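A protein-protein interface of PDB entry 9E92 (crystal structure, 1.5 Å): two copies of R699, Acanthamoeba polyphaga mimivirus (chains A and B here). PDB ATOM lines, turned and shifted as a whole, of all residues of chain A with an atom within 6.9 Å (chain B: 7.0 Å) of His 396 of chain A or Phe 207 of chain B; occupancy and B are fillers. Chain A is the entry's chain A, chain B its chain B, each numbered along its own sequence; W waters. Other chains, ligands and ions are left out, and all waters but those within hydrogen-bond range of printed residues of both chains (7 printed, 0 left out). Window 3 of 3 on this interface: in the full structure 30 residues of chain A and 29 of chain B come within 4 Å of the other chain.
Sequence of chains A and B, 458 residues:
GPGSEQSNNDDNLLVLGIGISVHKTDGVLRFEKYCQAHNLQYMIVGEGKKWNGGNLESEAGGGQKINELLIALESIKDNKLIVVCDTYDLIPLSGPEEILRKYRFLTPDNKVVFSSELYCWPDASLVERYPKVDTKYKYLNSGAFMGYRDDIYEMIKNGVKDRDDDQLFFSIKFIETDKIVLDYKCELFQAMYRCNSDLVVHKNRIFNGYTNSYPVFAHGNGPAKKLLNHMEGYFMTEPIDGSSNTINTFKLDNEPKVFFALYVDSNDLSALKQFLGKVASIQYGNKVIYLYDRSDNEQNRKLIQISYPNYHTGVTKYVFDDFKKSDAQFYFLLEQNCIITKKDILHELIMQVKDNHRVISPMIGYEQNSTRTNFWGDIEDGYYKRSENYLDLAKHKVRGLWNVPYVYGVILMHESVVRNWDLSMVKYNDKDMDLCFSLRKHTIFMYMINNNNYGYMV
Among the printed residues, merely in contact across the chains: Lys 397 of chain A with Phe 207 of chain B (3.2 Å), Lys 397 of chain A with Val 200 of chain B (3.7 Å), Val 398 of chain A with Val 200 of chain B (3.7 Å), His 396 of chain A with Phe 207 of chain B (3.8 Å), Arg 399 of chain A with Tyr 214 of chain B (3.9 Å), Val 398 of chain A with Phe 207 of chain B (3.9 Å), Arg 399 of chain A with Phe 207 of chain B (3.97 Å) and Val 398 of chain A with His 202 of chain B (3.98 Å).
The guanidinium group (NE) of Arg 399 of chain A sits close to the side-chain amide nitrogen (ND2) of Asn 212 of chain B (3.3 Å).
The backbone carbonyl oxygen of Asn 451 of chain A lies within hydrogen-bond range of the side-chain amide nitrogen of Asn 212 of chain B.
No position is printed for both chains.
Of the 10 pairs that touch across the chains among the printed residues, none has its exchanged pair printed and touching as well.
His 396 of chain A touches just one residue of chain B: Phe 207 (3.8 Å).
Of the printed residues of chain A, Phe 207 of chain B touches His 396 (3.8 Å), Lys 397 (3.2 Å), Val 398 (3.9 Å) and Arg 399 (3.97 Å).
Printed residues of chain B within 4 Å of Lys 397 of chain A: Val 200 and Phe 207.
Printed residues of chain B within 4 Å of Asn 451 of chain A: Asn 212 (3.3 Å).
Ser 213 of chain B touches none of the printed residues of chain A.
The nearest printed residue of chain B that does not touch Arg 399 of chain A is His 202 of chain B (4.3 Å).
Water W3 bridges O of Arg 399 of chain A (2.8 Å) and NE2 of His 202 of chain B (2.8 Å).
Water W5 lies within hydrogen-bond range of O of His 396 of chain A (2.8 Å), O of Gly 209 of chain B (2.8 Å) and NE of Arg 399 of chain A (2.8 Å).
Water W2 bridges the backbone carbonyl oxygen (O) of Asn 451 of chain A (2.9 Å) and the side-chain amide oxygen (OD1) of Asn 212 of chain B (3.2 Å).
Water W6 lies within hydrogen-bond range of the side-chain hydroxyl of Tyr 214 of chain B and the backbone NH of Arg 399 of chain A.
Water W1 lies within hydrogen-bond range of O of Gly 209 of chain B (2.9 Å), NH2 of Arg 399 of chain A (3.2 Å) and O of Tyr 210 of chain B (3.4 Å).
Hydrophobic or aromatic side chains of chain A within 4 Å of the printed part of chain B: Val 398.
Among the printed residues, 10 pairs touch across the chains.
The backbone carbonyl oxygen (O) of Asp 392 of chain A sits at hydrogen-bond distance from the backbone NH (N) of Lys 397 of chain A (2.8 Å).
The guanidinium group of Arg 399 of chain A lies within hydrogen-bond range of the backbone carbonyl oxygen of Asn 450 of chain A (3.0 Å).
The side-chain hydroxyl (OH) of Tyr 454 of chain A is in hydrogen-bond range of the backbone NH (N) of Asn 451 of chain A (3.4 Å).
O of Asn 451 of chain A lies within hydrogen-bond range of NH1 of Arg 399 of chain A, 3.3 Å away.
ND2 of Asn 450 of chain A is in hydrogen-bond range of O of Val 398 of chain A (3.1 Å).
NH2 of Arg 205 of chain B sits at hydrogen-bond distance from O of Tyr 214 of chain B (3.0 Å).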
ATOM      1  N   MET A 363     -19.981 -11.340 -13.086  1.00  0.00           N
ATOM      2  CA  MET A 363     -18.834 -12.000 -13.696  1.00  0.00           C
ATOM      3  C   MET A 363     -18.867 -13.503 -13.440  1.00  0.00           C
ATOM      4  O   MET A 363     -18.948 -13.916 -12.271  1.00  0.00           O
ATOM      5  CB  MET A 363     -17.551 -11.492 -13.049  1.00  0.00           C
ATOM      6  CG  MET A 363     -16.316 -11.886 -13.840  1.00  0.00           C
ATOM      7  SD  MET A 363     -14.760 -11.476 -12.969  1.00  0.00           S
ATOM      8  CE  MET A 363     -14.754 -12.757 -11.743  1.00  0.00           C
ATOM      9  N   TYR A 390      -7.205  -7.163 -15.701  1.00  0.00           N
ATOM     10  CA  TYR A 390      -8.147  -8.220 -16.061  1.00  0.00           C
ATOM     11  C   TYR A 390      -8.001  -9.463 -15.161  1.00  0.00           C
ATOM     12  O   TYR A 390      -8.978  -9.974 -14.591  1.00  0.00           O
ATOM     13  CB  TYR A 390      -8.045  -8.571 -17.557  1.00  0.00           C
ATOM     14  CG  TYR A 390      -8.954  -9.748 -17.887  1.00  0.00           C
ATOM     15  CD1 TYR A 390     -10.294  -9.552 -18.175  1.00  0.00           C
ATOM     16  CD2 TYR A 390      -8.498 -11.048 -17.777  1.00  0.00           C
ATOM     17  CE1 TYR A 390     -11.151 -10.622 -18.417  1.00  0.00           C
ATOM     18  CE2 TYR A 390      -9.353 -12.123 -17.961  1.00  0.00           C
ATOM     19  CZ  TYR A 390     -10.677 -11.908 -18.247  1.00  0.00           C
ATOM     20  OH  TYR A 390     -11.504 -13.012 -18.388  1.00  0.00           O
ATOM     21  N   LEU A 391      -6.788  -9.961 -14.993  1.00  0.00           N
ATOM     22  CA  LEU A 391      -6.578 -11.152 -14.183  1.00  0.00           C
ATOM     23  C   LEU A 391      -6.906 -10.911 -12.709  1.00  0.00           C
ATOM     24  O   LEU A 391      -7.457 -11.762 -12.026  1.00  0.00           O
ATOM     25  CB  LEU A 391      -5.153 -11.653 -14.407  1.00  0.00           C
ATOM     26  CG  LEU A 391      -4.881 -12.239 -15.795  1.00  0.00           C
ATOM     27  CD1 LEU A 391      -3.395 -12.617 -15.924  1.00  0.00           C
ATOM     28  CD2 LEU A 391      -5.761 -13.437 -16.171  1.00  0.00           C
ATOM     29  N   ASP A 392      -6.576  -9.711 -12.210  1.00  0.00           N
ATOM     30  CA  ASP A 392      -6.935  -9.348 -10.834  1.00  0.00           C
ATOM     31  C   ASP A 392      -8.443  -9.495 -10.624  1.00  0.00           C
ATOM     32  O   ASP A 392      -8.935 -10.035  -9.632  1.00  0.00           O
ATOM     33  CB  ASP A 392      -6.502  -7.946 -10.431  1.00  0.00           C
ATOM     34  CG  ASP A 392      -5.015  -7.701 -10.213  1.00  0.00           C
ATOM     35  OD1 ASP A 392      -4.296  -8.717 -10.111  1.00  0.00           O
ATOM     36  OD2 ASP A 392      -4.654  -6.487 -10.016  1.00  0.00           O
ATOM     37  N   LEU A 393      -9.208  -8.978 -11.572  1.00  0.00           N
ATOM     38  CA  LEU A 393     -10.653  -9.063 -11.489  1.00  0.00           C
ATOM     39  C   LEU A 393     -11.183 -10.501 -11.613  1.00  0.00           C
ATOM     40  O   LEU A 393     -12.027 -10.909 -10.811  1.00  0.00           O
ATOM     41  CB  LEU A 393     -11.277  -8.135 -12.538  1.00  0.00           C
ATOM     42  CG  LEU A 393     -11.027  -6.647 -12.371  1.00  0.00           C
ATOM     43  CD1 LEU A 393     -11.548  -5.830 -13.570  1.00  0.00           C
ATOM     44  CD2 LEU A 393     -11.536  -6.111 -11.123  1.00  0.00           C
ATOM     45  N   ALA A 394     -10.698 -11.258 -12.609  1.00  0.00           N
ATOM     46  CA  ALA A 394     -11.106 -12.629 -12.871  1.00  0.00           C
ATOM     47  C   ALA A 394     -10.803 -13.581 -11.697  1.00  0.00           C
ATOM     48  O   ALA A 394     -11.501 -14.581 -11.552  1.00  0.00           O
ATOM     49  CB  ALA A 394     -10.408 -13.091 -14.157  1.00  0.00           C
ATOM     50  N   LYS A 395      -9.763 -13.254 -10.909  1.00  0.00           N
ATOM     51  CA  LYS A 395      -9.367 -14.058  -9.747  1.00  0.00           C
ATOM     52  C   LYS A 395      -9.827 -13.425  -8.414  1.00  0.00           C
ATOM     53  O   LYS A 395      -9.498 -13.921  -7.322  1.00  0.00           O
ATOM     54  CB  LYS A 395      -7.845 -14.199  -9.733  1.00  0.00           C
ATOM     55  CG  LYS A 395      -7.303 -14.892 -10.981  1.00  0.00           C
ATOM     56  CD  LYS A 395      -5.777 -14.985 -10.967  1.00  0.00           C
ATOM     57  CE  LYS A 395      -5.275 -15.896 -12.061  1.00  0.00           C
ATOM     58  NZ  LYS A 395      -3.836 -15.693 -12.265  1.00  0.00           N
ATOM     59  N   HIS A 396     -10.663 -12.369  -8.483  1.00  0.00           N
ATOM     60  CA  HIS A 396     -11.244 -11.773  -7.302  1.00  0.00           C
ATOM     61  C   HIS A 396     -10.180 -11.197  -6.346  1.00  0.00           C
ATOM     62  O   HIS A 396     -10.448 -11.141  -5.142  1.00  0.00           O
ATOM     63  CB  HIS A 396     -12.227 -12.717  -6.585  1.00  0.00           C
ATOM     64  CG  HIS A 396     -13.325 -13.288  -7.416  1.00  0.00           C
ATOM     65  ND1 HIS A 396     -13.298 -14.525  -8.038  1.00  0.00           N
ATOM     66  CD2 HIS A 396     -14.486 -12.710  -7.803  1.00  0.00           C
ATOM     67  CE1 HIS A 396     -14.459 -14.714  -8.671  1.00  0.00           C
ATOM     68  NE2 HIS A 396     -15.192 -13.623  -8.553  1.00  0.00           N
ATOM     69  N   LYS A 397      -9.068 -10.681  -6.862  1.00  0.00           N
ATOM     70  CA  LYS A 397      -8.071 -10.013  -6.031  1.00  0.00           C
ATOM     71  C   LYS A 397      -8.632  -8.716  -5.459  1.00  0.00           C
ATOM     72  O   LYS A 397      -8.201  -8.290  -4.390  1.00  0.00           O
ATOM     73  CB  LYS A 397      -6.775  -9.754  -6.808  1.00  0.00           C
ATOM     74  CG  LYS A 397      -5.647  -9.106  -6.017  1.00  0.00           C
ATOM     75  CD  LYS A 397      -4.278  -9.183  -6.684  1.00  0.00           C
ATOM     76  CE  LYS A 397      -3.262  -8.483  -5.841  1.00  0.00           C
ATOM     77  NZ  LYS A 397      -2.064  -8.211  -6.638  1.00  0.00           N
ATOM     78  N   VAL A 398      -9.516  -8.051  -6.215  1.00  0.00           N
ATOM     79  CA  VAL A 398     -10.303  -6.922  -5.754  1.00  0.00           C
ATOM     80  C   VAL A 398     -11.735  -7.161  -6.267  1.00  0.00           C
ATOM     81  O   VAL A 398     -11.930  -7.869  -7.262  1.00  0.00           O
ATOM     82  CB  VAL A 398      -9.805  -5.522  -6.214  1.00  0.00           C
ATOM     83  CG1 VAL A 398      -8.547  -5.101  -5.429  1.00  0.00           C
ATOM     84  CG2 VAL A 398      -9.476  -5.504  -7.690  1.00  0.00           C
ATOM     85  N   ARG A 399     -12.731  -6.615  -5.581  1.00  0.00           N
ATOM     86  CA  ARG A 399     -14.139  -6.843  -5.901  1.00  0.00           C
ATOM     87  C   ARG A 399     -14.880  -5.504  -5.905  1.00  0.00           C
ATOM     88  O   ARG A 399     -14.488  -4.571  -5.167  1.00  0.00           O
ATOM     89  CB  ARG A 399     -14.823  -7.799  -4.927  1.00  0.00           C
ATOM     90  CG  ARG A 399     -14.276  -9.220  -5.014  1.00  0.00           C
ATOM     91  CD  ARG A 399     -14.998 -10.146  -4.099  1.00  0.00           C
ATOM     92  NE  ARG A 399     -14.459 -11.503  -3.977  1.00  0.00           N
ATOM     93  CZ  ARG A 399     -15.064 -12.613  -4.371  1.00  0.00           C
ATOM     94  NH1 ARG A 399     -16.207 -12.613  -5.089  1.00  0.00           N
ATOM     95  NH2 ARG A 399     -14.523 -13.777  -3.985  1.00  0.00           N
ATOM     96  N   ILE A 449     -19.814  -6.842 -12.259  1.00  0.00           N
ATOM     97  CA  ILE A 449     -19.800  -6.970 -10.804  1.00  0.00           C
ATOM     98  C   ILE A 449     -19.236  -8.340 -10.407  1.00  0.00           C
ATOM     99  O   ILE A 449     -19.648  -9.340 -10.993  1.00  0.00           O
ATOM    100  CB  ILE A 449     -21.177  -6.730 -10.184  1.00  0.00           C
ATOM    101  CG1 ILE A 449     -21.169  -6.770  -8.651  1.00  0.00           C
ATOM    102  CG2 ILE A 449     -22.254  -7.661 -10.718  1.00  0.00           C
ATOM    103  CD1 ILE A 449     -22.480  -6.330  -7.990  1.00  0.00           C
ATOM    104  N   ASN A 450     -18.288  -8.371  -9.470  1.00  0.00           N
ATOM    105  CA  ASN A 450     -17.629  -9.614  -9.048  1.00  0.00           C
ATOM    106  C   ASN A 450     -17.648  -9.783  -7.527  1.00  0.00           C
ATOM    107  O   ASN A 450     -16.734 -10.401  -6.977  1.00  0.00           O
ATOM    108  CB  ASN A 450     -16.217  -9.763  -9.645  1.00  0.00           C
ATOM    109  CG  ASN A 450     -15.230  -8.780  -9.071  1.00  0.00           C
ATOM    110  OD1 ASN A 450     -15.640  -7.741  -8.528  1.00  0.00           O
ATOM    111  ND2 ASN A 450     -13.934  -9.019  -9.262  1.00  0.00           N
ATOM    112  N   ASN A 451     -18.764  -9.435  -6.890  1.00  0.00           N
ATOM    113  CA  ASN A 451     -18.871  -9.414  -5.422  1.00  0.00           C
ATOM    114  C   ASN A 451     -19.003 -10.802  -4.814  1.00  0.00           C
ATOM    115  O   ASN A 451     -18.733 -10.990  -3.628  1.00  0.00           O
ATOM    116  CB  ASN A 451     -19.959  -8.464  -4.933  1.00  0.00           C
ATOM    117  CG  ASN A 451     -19.549  -7.026  -5.017  1.00  0.00           C
ATOM    118  OD1 ASN A 451     -18.368  -6.701  -5.182  1.00  0.00           O
ATOM    119  ND2 ASN A 451     -20.531  -6.133  -4.991  1.00  0.00           N
ATOM    120  N   ASN A 452     -19.544 -11.755  -5.570  1.00  0.00           N
ATOM    121  CA  ASN A 452     -19.861 -13.087  -5.095  1.00  0.00           C
ATOM    122  C   ASN A 452     -19.705 -14.126  -6.214  1.00  0.00           C
ATOM    123  O   ASN A 452     -19.331 -13.804  -7.346  1.00  0.00           O
ATOM    124  CB  ASN A 452     -21.285 -13.121  -4.534  1.00  0.00           C
ATOM    125  CG  ASN A 452     -21.419 -12.483  -3.164  1.00  0.00           C
ATOM    126  OD1 ASN A 452     -20.857 -13.013  -2.190  1.00  0.00           O
ATOM    127  ND2 ASN A 452     -22.058 -11.345  -3.089  1.00  0.00           N
ATOM    128  N   ASN A 453     -19.867 -15.409  -5.857  1.00  0.00           N
ATOM    129  CA  ASN A 453     -19.822 -16.518  -6.818  1.00  0.00           C
ATOM    130  C   ASN A 453     -21.200 -16.693  -7.451  1.00  0.00           C
ATOM    131  O   ASN A 453     -22.156 -17.079  -6.749  1.00  0.00           O
ATOM    132  CB  ASN A 453     -19.419 -17.802  -6.094  1.00  0.00           C
ATOM    133  CG  ASN A 453     -19.310 -18.996  -7.015  1.00  0.00           C
ATOM    134  OD1 ASN A 453     -19.257 -18.871  -8.236  1.00  0.00           O
ATOM    135  ND2 ASN A 453     -19.335 -20.180  -6.422  1.00  0.00           N
ATOM    136  N   TYR A 454     -21.361 -16.342  -8.733  1.00  0.00           N
ATOM    137  CA  TYR A 454     -22.665 -16.246  -9.355  1.00  0.00           C
ATOM    138  C   TYR A 454     -23.059 -17.449 -10.222  1.00  0.00           C
ATOM    139  O   TYR A 454     -24.255 -17.687 -10.406  1.00  0.00           O
ATOM    140  CB  TYR A 454     -22.710 -14.965 -10.215  1.00  0.00           C
ATOM    141  CG  TYR A 454     -22.507 -13.657  -9.460  1.00  0.00           C
ATOM    142  CD1 TYR A 454     -23.348 -13.331  -8.427  1.00  0.00           C
ATOM    143  CD2 TYR A 454     -21.466 -12.796  -9.729  1.00  0.00           C
ATOM    144  CE1 TYR A 454     -23.176 -12.162  -7.699  1.00  0.00           C
ATOM    145  CE2 TYR A 454     -21.274 -11.610  -9.026  1.00  0.00           C
ATOM    146  CZ  TYR A 454     -22.166 -11.298  -8.017  1.00  0.00           C
ATOM    147  OH  TYR A 454     -22.031 -10.141  -7.285  1.00  0.00           O
ATOM    148  N   GLN B 190      -7.304  -8.386  11.280  1.00  0.00           N
ATOM    149  CA  GLN B 190      -6.330  -9.035  10.415  1.00  0.00           C
ATOM    150  C   GLN B 190      -4.948  -9.145  11.051  1.00  0.00           C
ATOM    151  O   GLN B 190      -4.271  -8.122  11.218  1.00  0.00           O
ATOM    152  CB  GLN B 190      -6.177  -8.265   9.091  1.00  0.00           C
ATOM    153  CG  GLN B 190      -5.203  -8.889   8.099  1.00  0.00           C
ATOM    154  CD  GLN B 190      -5.757 -10.130   7.404  1.00  0.00           C
ATOM    155  OE1 GLN B 190      -6.842 -10.073   6.866  1.00  0.00           O
ATOM    156  NE2 GLN B 190      -5.014 -11.204   7.416  1.00  0.00           N
ATOM    157  N   ASP B 198      -2.622 -12.425   0.329  1.00  0.00           N
ATOM    158  CA  ASP B 198      -4.068 -12.293   0.498  1.00  0.00           C
ATOM    159  C   ASP B 198      -4.486 -10.812   0.428  1.00  0.00           C
ATOM    160  O   ASP B 198      -5.682 -10.513   0.233  1.00  0.00           O
ATOM    161  CB  ASP B 198      -4.558 -12.837   1.827  1.00  0.00           C
ATOM    162  CG  ASP B 198      -4.361 -14.317   2.147  1.00  0.00           C
ATOM    163  OD1 ASP B 198      -4.097 -15.083   1.208  1.00  0.00           O
ATOM    164  OD2 ASP B 198      -4.504 -14.662   3.367  1.00  0.00           O
ATOM    165  N   LEU B 199      -3.567  -9.879   0.709  1.00  0.00           N
ATOM    166  CA  LEU B 199      -3.928  -8.504   1.048  1.00  0.00           C
ATOM    167  C   LEU B 199      -3.564  -7.496  -0.029  1.00  0.00           C
ATOM    168  O   LEU B 199      -2.448  -7.538  -0.591  1.00  0.00           O
ATOM    169  CB  LEU B 199      -3.276  -8.105   2.374  1.00  0.00           C
ATOM    170  CG  LEU B 199      -3.459  -9.059   3.557  1.00  0.00           C
ATOM    171  CD1 LEU B 199      -2.711  -8.517   4.816  1.00  0.00           C
ATOM    172  CD2 LEU B 199      -4.908  -9.278   3.866  1.00  0.00           C
ATOM    173  N   VAL B 200      -4.452  -6.534  -0.252  1.00  0.00           N
ATOM    174  CA  VAL B 200      -4.154  -5.431  -1.150  1.00  0.00           C
ATOM    175  C   VAL B 200      -4.779  -4.160  -0.585  1.00  0.00           C
ATOM    176  O   VAL B 200      -5.837  -4.174   0.063  1.00  0.00           O
ATOM    177  CB  VAL B 200      -4.648  -5.696  -2.586  1.00  0.00           C
ATOM    178  CG1 VAL B 200      -6.175  -5.734  -2.619  1.00  0.00           C
ATOM    179  CG2 VAL B 200      -4.105  -4.714  -3.610  1.00  0.00           C
ATOM    180  N   VAL B 201      -4.108  -3.031  -0.836  1.00  0.00           N
ATOM    181  CA  VAL B 201      -4.645  -1.698  -0.579  1.00  0.00           C
ATOM    182  C   VAL B 201      -5.613  -1.303  -1.696  1.00  0.00           C
ATOM    183  O   VAL B 201      -5.258  -1.332  -2.865  1.00  0.00           O
ATOM    184  CB  VAL B 201      -3.538  -0.645  -0.336  1.00  0.00           C
ATOM    185  CG1 VAL B 201      -4.121   0.721  -0.097  1.00  0.00           C
ATOM    186  CG2 VAL B 201      -2.635  -1.083   0.817  1.00  0.00           C
ATOM    187  N   HIS B 202      -6.834  -0.968  -1.300  1.00  0.00           N
ATOM    188  CA  HIS B 202      -7.915  -0.622  -2.231  1.00  0.00           C
ATOM    189  C   HIS B 202      -8.867   0.336  -1.524  1.00  0.00           C
ATOM    190  O   HIS B 202      -9.348   0.064  -0.397  1.00  0.00           O
ATOM    191  CB  HIS B 202      -8.618  -1.890  -2.671  1.00  0.00           C
ATOM    192  CG  HIS B 202      -9.631  -1.642  -3.735  1.00  0.00           C
ATOM    193  ND1 HIS B 202      -9.249  -1.212  -4.995  1.00  0.00           N
ATOM    194  CD2 HIS B 202     -10.973  -1.825  -3.751  1.00  0.00           C
ATOM    195  CE1 HIS B 202     -10.374  -1.164  -5.738  1.00  0.00           C
ATOM    196  NE2 HIS B 202     -11.429  -1.510  -5.009  1.00  0.00           N
ATOM    197  N   ARG B 205      -8.458   1.144   2.193  1.00  0.00           N
ATOM    198  CA  ARG B 205      -8.647  -0.021   3.065  1.00  0.00           C
ATOM    199  C   ARG B 205      -7.712  -1.160   2.695  1.00  0.00           C
ATOM    200  O   ARG B 205      -7.114  -1.167   1.593  1.00  0.00           O
ATOM    201  CB  ARG B 205     -10.081  -0.542   2.920  1.00  0.00           C
ATOM    202  CG  ARG B 205     -11.163   0.436   3.362  1.00  0.00           C
ATOM    203  CD  ARG B 205     -11.186   0.684   4.886  1.00  0.00           C
ATOM    204  NE  ARG B 205     -11.508  -0.500   5.715  1.00  0.00           N
ATOM    205  CZ  ARG B 205     -12.687  -0.780   6.196  1.00  0.00           C
ATOM    206  NH1 ARG B 205     -13.707   0.011   5.994  1.00  0.00           N
ATOM    207  NH2 ARG B 205     -12.857  -1.870   6.920  1.00  0.00           N
ATOM    208  N   ILE B 206      -7.557  -2.134   3.610  1.00  0.00           N
ATOM    209  CA  ILE B 206      -7.030  -3.443   3.217  1.00  0.00           C
ATOM    210  C   ILE B 206      -8.207  -4.323   2.796  1.00  0.00           C
ATOM    211  O   ILE B 206      -9.193  -4.476   3.536  1.00  0.00           O
ATOM    212  CB  ILE B 206      -6.251  -4.096   4.362  1.00  0.00           C
ATOM    213  CG1 ILE B 206      -5.006  -3.288   4.707  1.00  0.00           C
ATOM    214  CG2 ILE B 206      -5.984  -5.558   4.072  1.00  0.00           C
ATOM    215  CD1 ILE B 206      -4.203  -3.819   5.886  1.00  0.00           C
ATOM    216  N   PHE B 207      -8.078  -4.955   1.630  1.00  0.00           N
ATOM    217  CA  PHE B 207      -8.979  -6.011   1.154  1.00  0.00           C
ATOM    218  C   PHE B 207      -8.233  -7.352   1.225  1.00  0.00           C
ATOM    219  O   PHE B 207      -7.138  -7.491   0.670  1.00  0.00           O
ATOM    220  CB  PHE B 207      -9.461  -5.714  -0.272  1.00  0.00           C
ATOM    221  CG  PHE B 207     -10.423  -6.793  -0.776  1.00  0.00           C
ATOM    222  CD1 PHE B 207     -11.674  -6.970  -0.207  1.00  0.00           C
ATOM    223  CD2 PHE B 207     -10.061  -7.630  -1.820  1.00  0.00           C
ATOM    224  CE1 PHE B 207     -12.520  -7.960  -0.671  1.00  0.00           C
ATOM    225  CE2 PHE B 207     -10.911  -8.623  -2.281  1.00  0.00           C
ATOM    226  CZ  PHE B 207     -12.128  -8.785  -1.704  1.00  0.00           C
ATOM    227  N   ASN B 208      -8.874  -8.317   1.879  1.00  0.00           N
ATOM    228  CA  ASN B 208      -8.401  -9.687   1.978  1.00  0.00           C
ATOM    229  C   ASN B 208      -9.177 -10.516   0.957  1.00  0.00           C
ATOM    230  O   ASN B 208     -10.376 -10.742   1.111  1.00  0.00           O
ATOM    231  CB  ASN B 208      -8.593 -10.210   3.384  1.00  0.00           C
ATOM    232  CG  ASN B 208      -8.024 -11.610   3.579  1.00  0.00           C
ATOM    233  OD1 ASN B 208      -8.027 -12.434   2.656  1.00  0.00           O
ATOM    234  ND2 ASN B 208      -7.494 -11.911   4.762  1.00  0.00           N
ATOM    235  N   GLY B 209      -8.505 -10.869  -0.125  1.00  0.00           N
ATOM    236  CA  GLY B 209      -9.142 -11.640  -1.199  1.00  0.00           C
ATOM    237  C   GLY B 209      -9.350 -13.100  -0.873  1.00  0.00           C
ATOM    238  O   GLY B 209     -10.134 -13.767  -1.556  1.00  0.00           O
ATOM    239  N   TYR B 210      -8.617 -13.634   0.094  1.00  0.00           N
ATOM    240  CA  TYR B 210      -8.865 -15.012   0.503  1.00  0.00           C
ATOM    241  C   TYR B 210     -10.182 -15.142   1.247  1.00  0.00           C
ATOM    242  O   TYR B 210     -10.943 -16.105   0.998  1.00  0.00           O
ATOM    243  CB  TYR B 210      -7.682 -15.500   1.352  1.00  0.00           C
ATOM    244  CG  TYR B 210      -7.751 -16.925   1.893  1.00  0.00           C
ATOM    245  CD1 TYR B 210      -8.425 -17.224   3.084  1.00  0.00           C
ATOM    246  CD2 TYR B 210      -7.152 -17.974   1.215  1.00  0.00           C
ATOM    247  CE1 TYR B 210      -8.482 -18.517   3.590  1.00  0.00           C
ATOM    248  CE2 TYR B 210      -7.166 -19.266   1.732  1.00  0.00           C
ATOM    249  CZ  TYR B 210      -7.837 -19.530   2.905  1.00  0.00           C
ATOM    250  OH  TYR B 210      -7.871 -20.829   3.439  1.00  0.00           O
ATOM    251  N   THR B 211     -10.477 -14.199   2.160  1.00  0.00           N
ATOM    252  CA  THR B 211     -11.694 -14.240   2.950  1.00  0.00           C
ATOM    253  C   THR B 211     -12.841 -13.445   2.307  1.00  0.00           C
ATOM    254  O   THR B 211     -13.983 -13.592   2.772  1.00  0.00           O
ATOM    255  CB  THR B 211     -11.409 -13.648   4.325  1.00  0.00           C
ATOM    256  OG1 THR B 211     -10.947 -12.312   4.189  1.00  0.00           O
ATOM    257  CG2 THR B 211     -10.399 -14.446   5.101  1.00  0.00           C
ATOM    258  N   ASN B 212     -12.542 -12.579   1.321  1.00  0.00           N
ATOM    259  CA  ASN B 212     -13.530 -11.619   0.785  1.00  0.00           C
ATOM    260  C   ASN B 212     -14.042 -10.716   1.912  1.00  0.00           C
ATOM    261  O   ASN B 212     -15.235 -10.676   2.227  1.00  0.00           O
ATOM    262  CB  ASN B 212     -14.660 -12.325   0.042  1.00  0.00           C
ATOM    263  CG  ASN B 212     -15.547 -11.395  -0.755  1.00  0.00           C
ATOM    264  OD1 ASN B 212     -15.318 -10.186  -0.813  1.00  0.00           O
ATOM    265  ND2 ASN B 212     -16.535 -12.002  -1.425  1.00  0.00           N
ATOM    266  N   SER B 213     -13.129  -9.942   2.511  1.00  0.00           N
ATOM    267  CA  SER B 213     -13.440  -9.040   3.610  1.00  0.00           C
ATOM    268  C   SER B 213     -12.540  -7.794   3.556  1.00  0.00           C
ATOM    269  O   SER B 213     -11.464  -7.768   2.910  1.00  0.00           O
ATOM    270  CB  SER B 213     -13.271  -9.754   4.936  1.00  0.00           C
ATOM    271  OG  SER B 213     -11.864  -9.979   5.240  1.00  0.00           O
ATOM    272  N   TYR B 214     -12.986  -6.759   4.254  1.00  0.00           N
ATOM    273  CA  TYR B 214     -12.226  -5.531   4.521  1.00  0.00           C
ATOM    274  C   TYR B 214     -12.030  -5.442   6.031  1.00  0.00           C
ATOM    275  O   TYR B 214     -12.838  -4.873   6.752  1.00  0.00           O
ATOM    276  CB  TYR B 214     -12.939  -4.280   4.004  1.00  0.00           C
ATOM    277  CG  TYR B 214     -13.115  -4.094   2.503  1.00  0.00           C
ATOM    278  CD1 TYR B 214     -12.101  -3.521   1.761  1.00  0.00           C
ATOM    279  CD2 TYR B 214     -14.271  -4.499   1.842  1.00  0.00           C
ATOM    280  CE1 TYR B 214     -12.271  -3.253   0.410  1.00  0.00           C
ATOM    281  CE2 TYR B 214     -14.435  -4.249   0.484  1.00  0.00           C
ATOM    282  CZ  TYR B 214     -13.419  -3.643  -0.237  1.00  0.00           C
ATOM    283  OH  TYR B 214     -13.516  -3.336  -1.618  1.00  0.00           O
ATOM    284  N   PRO B 215     -10.948  -6.062   6.582  1.00  0.00           N
ATOM    285  CA  PRO B 215     -10.773  -6.088   8.027  1.00  0.00           C
ATOM    286  C   PRO B 215     -10.685  -4.688   8.627  1.00  0.00           C
ATOM    287  O   PRO B 215     -10.043  -3.786   8.072  1.00  0.00           O
ATOM    288  CB  PRO B 215      -9.416  -6.895   8.225  1.00  0.00           C
ATOM    289  CG  PRO B 215      -8.718  -6.809   6.884  1.00  0.00           C
ATOM    290  CD  PRO B 215      -9.873  -6.814   5.888  1.00  0.00           C
HETATM  291  O   HOH W   1     -12.765 -15.064  -1.672  1.00  0.00           O
HETATM  292  O   HOH W   2     -17.785  -8.718  -2.179  1.00  0.00           O
HETATM  293  O   HOH W   3     -14.164  -1.881  -5.644  1.00  0.00           O
HETATM  294  O   HOH W   4     -16.003  -3.239  -2.554  1.00  0.00           O
HETATM  295  O   HOH W   5     -11.896 -12.213  -3.053  1.00  0.00           O
HETATM  296  O   HOH W   6     -11.996  -5.253  -3.138  1.00  0.00           O
HETATM  297  O   HOH W   7      -6.700  -9.389  -2.349  1.00  0.00           O
